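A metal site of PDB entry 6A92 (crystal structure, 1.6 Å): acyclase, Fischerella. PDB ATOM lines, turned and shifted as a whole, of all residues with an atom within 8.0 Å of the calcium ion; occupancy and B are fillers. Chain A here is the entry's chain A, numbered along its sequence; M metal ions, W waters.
The backbone carbonyl oxygen (O) of Asn 137 lies within hydrogen-bond range of the backbone NH (N) of Gly 176 (2.7 Å).
The backbone carbonyl oxygen (O) of Ala 148 lies within hydrogen-bond range of the backbone NH (N) of Phe 210 (2.9 Å).
The side-chain amide nitrogen (ND2) of Asn 137 is in hydrogen-bond range of the backbone carbonyl oxygen (O) of Ile 173, 3.0 Å away.
The backbone NH of Asn 137 lies within hydrogen-bond range of the backbone carbonyl oxygen of Glu 177 (3.1 Å).
The backbone carbonyl oxygen (O) of Gly 140 lies within hydrogen-bond range of the backbone NH (N) of Phe 147, 2.9 Å away.
The backbone NH (N) of Ala 148 sits at hydrogen-bond distance from the side-chain hydroxyl (OG) of Ser 146, at 3.3 Å.
C of Ala 148 touches the calcium ion (3.8 Å).
Of the 22 residues printed, 6 come within 4 Å of the calcium ion.
Along chain A the residues within 4 Å of the calcium ion span positions 137 to 175.
The nearest printed residue that does not touch the calcium ion is Ala 139 (4.4 Å).
The calcium ion is bound by the backbone carbonyl oxygen (O) of Leu 138 (2.2 Å), the backbone carbonyl oxygen (O) of Phe 147 (2.3 Å), the side-chain amide oxygen (OD1) of Asn 137 (2.3 Å), the backbone carbonyl oxygen (O) of Gly 149 (2.3 Å) and the side-chain carboxylate (OE1) of Glu 175 (2.5 Å).
The calcium ion has five donor atoms within binding distance.
Slightly farther from the calcium ion lies water W1 (2.9 Å).
Water W1 bridges the backbone carbonyl oxygen of Gly 212 and the backbone NH of Leu 138.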
ATOM      1  N   PHE A  88      11.002  18.720  26.705  1.00  0.00           N
ATOM      2  CA  PHE A  88      11.206  20.112  26.316  1.00  0.00           C
ATOM      3  C   PHE A  88      11.417  20.998  27.568  1.00  0.00           C
ATOM      4  O   PHE A  88      11.759  22.182  27.422  1.00  0.00           O
ATOM      5  CB  PHE A  88      10.069  20.516  25.357  1.00  0.00           C
ATOM      6  CG  PHE A  88       9.974  19.682  24.097  1.00  0.00           C
ATOM      7  CD1 PHE A  88      11.101  19.406  23.339  1.00  0.00           C
ATOM      8  CD2 PHE A  88       8.764  19.129  23.696  1.00  0.00           C
ATOM      9  CE1 PHE A  88      11.024  18.590  22.220  1.00  0.00           C
ATOM     10  CE2 PHE A  88       8.685  18.327  22.573  1.00  0.00           C
ATOM     11  CZ  PHE A  88       9.812  18.069  21.824  1.00  0.00           C
ATOM     12  N   GLY A 136       7.488  30.510  29.975  1.00  0.00           N
ATOM     13  CA  GLY A 136       8.426  29.385  29.818  1.00  0.00           C
ATOM     14  C   GLY A 136       9.207  29.447  28.526  1.00  0.00           C
ATOM     15  O   GLY A 136       8.690  29.934  27.486  1.00  0.00           O
ATOM     16  N   ASN A 137      10.438  28.962  28.607  1.00  0.00           N
ATOM     17  CA  ASN A 137      11.408  28.902  27.546  1.00  0.00           C
ATOM     18  C   ASN A 137      11.634  27.408  27.254  1.00  0.00           C
ATOM     19  O   ASN A 137      12.060  26.662  28.114  1.00  0.00           O
ATOM     20  CB  ASN A 137      12.708  29.599  27.977  1.00  0.00           C
ATOM     21  CG  ASN A 137      13.788  29.644  26.913  1.00  0.00           C
ATOM     22  OD1 ASN A 137      13.582  29.125  25.820  1.00  0.00           O
ATOM     23  ND2 ASN A 137      14.934  30.218  27.245  1.00  0.00           N
ATOM     24  N   LEU A 138      11.271  26.973  26.053  1.00  0.00           N
ATOM     25  CA  LEU A 138      11.402  25.547  25.712  1.00  0.00           C
ATOM     26  C   LEU A 138      12.875  25.184  25.523  1.00  0.00           C
ATOM     27  O   LEU A 138      13.631  25.960  24.989  1.00  0.00           O
ATOM     28  CB  LEU A 138      10.697  25.298  24.387  1.00  0.00           C
ATOM     29  CG  LEU A 138       9.179  25.230  24.449  1.00  0.00           C
ATOM     30  CD1 LEU A 138       8.613  26.633  24.433  1.00  0.00           C
ATOM     31  CD2 LEU A 138       8.672  24.438  23.257  1.00  0.00           C
ATOM     32  N   ALA A 139      13.209  23.926  25.793  1.00  0.00           N
ATOM     33  CA  ALA A 139      14.576  23.448  25.625  1.00  0.00           C
ATOM     34  C   ALA A 139      14.551  22.227  24.713  1.00  0.00           C
ATOM     35  O   ALA A 139      13.508  21.590  24.556  1.00  0.00           O
ATOM     36  CB  ALA A 139      15.184  23.067  26.949  1.00  0.00           C
ATOM     37  N   GLY A 140      15.711  21.934  24.167  1.00  0.00           N
ATOM     38  CA  GLY A 140      15.957  20.648  23.533  1.00  0.00           C
ATOM     39  C   GLY A 140      15.925  20.686  22.014  1.00  0.00           C
ATOM     40  O   GLY A 140      16.073  21.728  21.405  1.00  0.00           O
ATOM     41  N   SER A 146      15.476  22.631  16.479  1.00  0.00           N
ATOM     42  CA  SER A 146      16.127  23.114  17.671  1.00  0.00           C
ATOM     43  C   SER A 146      15.180  24.066  18.413  1.00  0.00           C
ATOM     44  O   SER A 146      14.658  24.980  17.792  1.00  0.00           O
ATOM     45  CB  SER A 146      17.420  23.800  17.349  1.00  0.00           C
ATOM     46  OG  SER A 146      17.972  24.349  18.536  1.00  0.00           O
ATOM     47  N   PHE A 147      15.075  23.898  19.735  1.00  0.00           N
ATOM     48  CA  PHE A 147      14.257  24.799  20.562  1.00  0.00           C
ATOM     49  C   PHE A 147      15.145  25.760  21.355  1.00  0.00           C
ATOM     50  O   PHE A 147      14.622  26.544  22.167  1.00  0.00           O
ATOM     51  CB  PHE A 147      13.347  24.026  21.502  1.00  0.00           C
ATOM     52  CG  PHE A 147      12.452  23.073  20.738  1.00  0.00           C
ATOM     53  CD1 PHE A 147      11.434  23.560  19.956  1.00  0.00           C
ATOM     54  CD2 PHE A 147      12.727  21.722  20.678  1.00  0.00           C
ATOM     55  CE1 PHE A 147      10.594  22.729  19.241  1.00  0.00           C
ATOM     56  CE2 PHE A 147      11.916  20.881  19.941  1.00  0.00           C
ATOM     57  CZ  PHE A 147      10.838  21.379  19.245  1.00  0.00           C
ATOM     58  N   ALA A 148      16.429  25.779  21.042  1.00  0.00           N
ATOM     59  CA  ALA A 148      17.357  26.728  21.685  1.00  0.00           C
ATOM     60  C   ALA A 148      16.991  28.159  21.314  1.00  0.00           C
ATOM     61  O   ALA A 148      16.671  28.492  20.193  1.00  0.00           O
ATOM     62  CB  ALA A 148      18.782  26.438  21.281  1.00  0.00           C
ATOM     63  N   GLY A 149      16.996  29.027  22.326  1.00  0.00           N
ATOM     64  CA  GLY A 149      16.624  30.420  22.097  1.00  0.00           C
ATOM     65  C   GLY A 149      15.213  30.733  22.543  1.00  0.00           C
ATOM     66  O   GLY A 149      14.443  29.872  22.912  1.00  0.00           O
ATOM     67  N   PHE A 150      14.866  32.020  22.483  1.00  0.00           N
ATOM     68  CA  PHE A 150      13.657  32.514  23.116  1.00  0.00           C
ATOM     69  C   PHE A 150      13.305  33.824  22.410  1.00  0.00           C
ATOM     70  O   PHE A 150      14.203  34.599  22.086  1.00  0.00           O
ATOM     71  CB  PHE A 150      13.931  32.734  24.602  1.00  0.00           C
ATOM     72  CG  PHE A 150      12.757  33.230  25.411  1.00  0.00           C
ATOM     73  CD1 PHE A 150      11.753  32.363  25.778  1.00  0.00           C
ATOM     74  CD2 PHE A 150      12.634  34.571  25.811  1.00  0.00           C
ATOM     75  CE1 PHE A 150      10.684  32.762  26.541  1.00  0.00           C
ATOM     76  CE2 PHE A 150      11.585  34.963  26.634  1.00  0.00           C
ATOM     77  CZ  PHE A 150      10.588  34.088  26.973  1.00  0.00           C
ATOM     78  N   PRO A 151      12.024  34.085  22.101  1.00  0.00           N
ATOM     79  CA  PRO A 151      11.669  35.239  21.261  1.00  0.00           C
ATOM     80  C   PRO A 151      11.431  36.538  22.025  1.00  0.00           C
ATOM     81  O   PRO A 151      11.227  37.553  21.425  1.00  0.00           O
ATOM     82  CB  PRO A 151      10.349  34.812  20.605  1.00  0.00           C
ATOM     83  CG  PRO A 151       9.719  33.879  21.614  1.00  0.00           C
ATOM     84  CD  PRO A 151      10.894  33.171  22.265  1.00  0.00           C
ATOM     85  N   ILE A 173      14.835  34.003  31.460  1.00  0.00           N
ATOM     86  CA  ILE A 173      14.255  32.682  31.619  1.00  0.00           C
ATOM     87  C   ILE A 173      15.172  31.659  30.972  1.00  0.00           C
ATOM     88  O   ILE A 173      15.464  31.719  29.808  1.00  0.00           O
ATOM     89  CB  ILE A 173      12.848  32.664  31.014  1.00  0.00           C
ATOM     90  CG1 ILE A 173      12.012  33.840  31.562  1.00  0.00           C
ATOM     91  CG2 ILE A 173      12.189  31.325  31.247  1.00  0.00           C
ATOM     92  CD1 ILE A 173      10.782  34.035  30.790  1.00  0.00           C
ATOM     93  N   LYS A 174      15.700  30.775  31.799  1.00  0.00           N
ATOM     94  CA  LYS A 174      16.648  29.758  31.365  1.00  0.00           C
ATOM     95  C   LYS A 174      15.937  28.776  30.447  1.00  0.00           C
ATOM     96  O   LYS A 174      14.738  28.570  30.581  1.00  0.00           O
ATOM     97  CB  LYS A 174      17.216  29.009  32.570  1.00  0.00           C
ATOM     98  CG  LYS A 174      18.185  29.798  33.442  1.00  0.00           C
ATOM     99  CD  LYS A 174      18.617  29.030  34.676  1.00  0.00           C
ATOM    100  CE  LYS A 174      19.568  29.804  35.555  1.00  0.00           C
ATOM    101  NZ  LYS A 174      19.310  29.507  36.991  1.00  0.00           N
ATOM    102  N   GLU A 175      16.711  28.123  29.570  1.00  0.00           N
ATOM    103  CA  GLU A 175      16.172  27.086  28.682  1.00  0.00           C
ATOM    104  C   GLU A 175      15.572  25.977  29.552  1.00  0.00           C
ATOM    105  O   GLU A 175      16.253  25.459  30.442  1.00  0.00           O
ATOM    106  CB  GLU A 175      17.279  26.472  27.816  1.00  0.00           C
ATOM    107  CG  GLU A 175      17.999  27.432  26.893  1.00  0.00           C
ATOM    108  CD  GLU A 175      17.216  27.889  25.676  1.00  0.00           C
ATOM    109  OE1 GLU A 175      16.359  27.153  25.193  1.00  0.00           O
ATOM    110  OE2 GLU A 175      17.517  28.963  25.165  1.00  0.00           O
ATOM    111  N   GLY A 176      14.317  25.634  29.266  1.00  0.00           N
ATOM    112  CA  GLY A 176      13.616  24.539  29.947  1.00  0.00           C
ATOM    113  C   GLY A 176      13.000  24.899  31.281  1.00  0.00           C
ATOM    114  O   GLY A 176      12.603  23.996  32.021  1.00  0.00           O
ATOM    115  N   GLU A 177      12.867  26.199  31.583  1.00  0.00           N
ATOM    116  CA  GLU A 177      12.265  26.610  32.838  1.00  0.00           C
ATOM    117  C   GLU A 177      11.159  27.649  32.622  1.00  0.00           C
ATOM    118  O   GLU A 177      11.024  28.190  31.523  1.00  0.00           O
ATOM    119  CB  GLU A 177      13.316  27.196  33.786  1.00  0.00           C
ATOM    120  CG  GLU A 177      14.443  26.244  34.075  1.00  0.00           C
ATOM    121  CD  GLU A 177      15.397  26.692  35.155  1.00  0.00           C
ATOM    122  OE1 GLU A 177      16.422  25.982  35.335  1.00  0.00           O
ATOM    123  OE2 GLU A 177      15.129  27.746  35.825  1.00  0.00           O
ATOM    124  N   LYS A 209      15.020  33.723  17.707  1.00  0.00           N
ATOM    125  CA  LYS A 209      14.634  32.336  17.476  1.00  0.00           C
ATOM    126  C   LYS A 209      15.379  31.486  18.493  1.00  0.00           C
ATOM    127  O   LYS A 209      16.482  31.880  18.892  1.00  0.00           O
ATOM    128  CB  LYS A 209      15.073  31.910  16.064  1.00  0.00           C
ATOM    129  CG  LYS A 209      14.215  32.430  14.938  1.00  0.00           C
ATOM    130  CD  LYS A 209      14.765  32.073  13.572  1.00  0.00           C
ATOM    131  CE  LYS A 209      14.190  32.977  12.503  1.00  0.00           C
ATOM    132  NZ  LYS A 209      13.435  32.243  11.468  1.00  0.00           N
ATOM    133  N   PHE A 210      14.886  30.308  18.865  1.00  0.00           N
ATOM    134  CA  PHE A 210      13.587  29.704  18.581  1.00  0.00           C
ATOM    135  C   PHE A 210      12.428  30.637  18.970  1.00  0.00           C
ATOM    136  O   PHE A 210      12.444  31.176  20.099  1.00  0.00           O
ATOM    137  CB  PHE A 210      13.504  28.393  19.373  1.00  0.00           C
ATOM    138  CG  PHE A 210      12.154  27.718  19.382  1.00  0.00           C
ATOM    139  CD1 PHE A 210      11.663  27.121  18.228  1.00  0.00           C
ATOM    140  CD2 PHE A 210      11.354  27.705  20.510  1.00  0.00           C
ATOM    141  CE1 PHE A 210      10.398  26.554  18.206  1.00  0.00           C
ATOM    142  CE2 PHE A 210      10.116  27.101  20.499  1.00  0.00           C
ATOM    143  CZ  PHE A 210       9.615  26.584  19.340  1.00  0.00           C
ATOM    144  N   SER A 211      11.413  30.711  18.118  1.00  0.00           N
ATOM    145  CA  SER A 211      10.375  31.772  18.172  1.00  0.00           C
ATOM    146  C   SER A 211       9.063  31.266  18.781  1.00  0.00           C
ATOM    147  O   SER A 211       7.988  31.712  18.410  1.00  0.00           O
ATOM    148  CB  SER A 211      10.162  32.375  16.790  1.00  0.00           C
ATOM    149  OG  SER A 211      11.321  33.056  16.379  1.00  0.00           O
ATOM    150  N   GLY A 212       9.138  30.343  19.746  1.00  0.00           N
ATOM    151  CA  GLY A 212       7.992  29.898  20.488  1.00  0.00           C
ATOM    152  C   GLY A 212       8.206  30.207  21.974  1.00  0.00           C
ATOM    153  O   GLY A 212       9.330  30.224  22.453  1.00  0.00           O
ATOM    154  N   LEU A 213       7.113  30.316  22.710  1.00  0.00           N
ATOM    155  CA  LEU A 213       7.182  30.422  24.168  1.00  0.00           C
ATOM    156  C   LEU A 213       5.852  29.995  24.774  1.00  0.00           C
ATOM    157  O   LEU A 213       4.824  29.913  24.074  1.00  0.00           O
ATOM    158  CB  LEU A 213       7.616  31.783  24.717  1.00  0.00           C
ATOM    159  CG  LEU A 213       7.089  33.118  24.217  1.00  0.00           C
ATOM    160  CD1 LEU A 213       5.741  33.155  23.639  1.00  0.00           C
ATOM    161  CD2 LEU A 213       7.197  34.158  25.294  1.00  0.00           C
HETATM  162 CA    CA M   1      14.303  27.819  24.037  1.00  0.00          CA
HETATM  163  O   HOH W   1      11.645  29.016  23.878  1.00  0.00           O
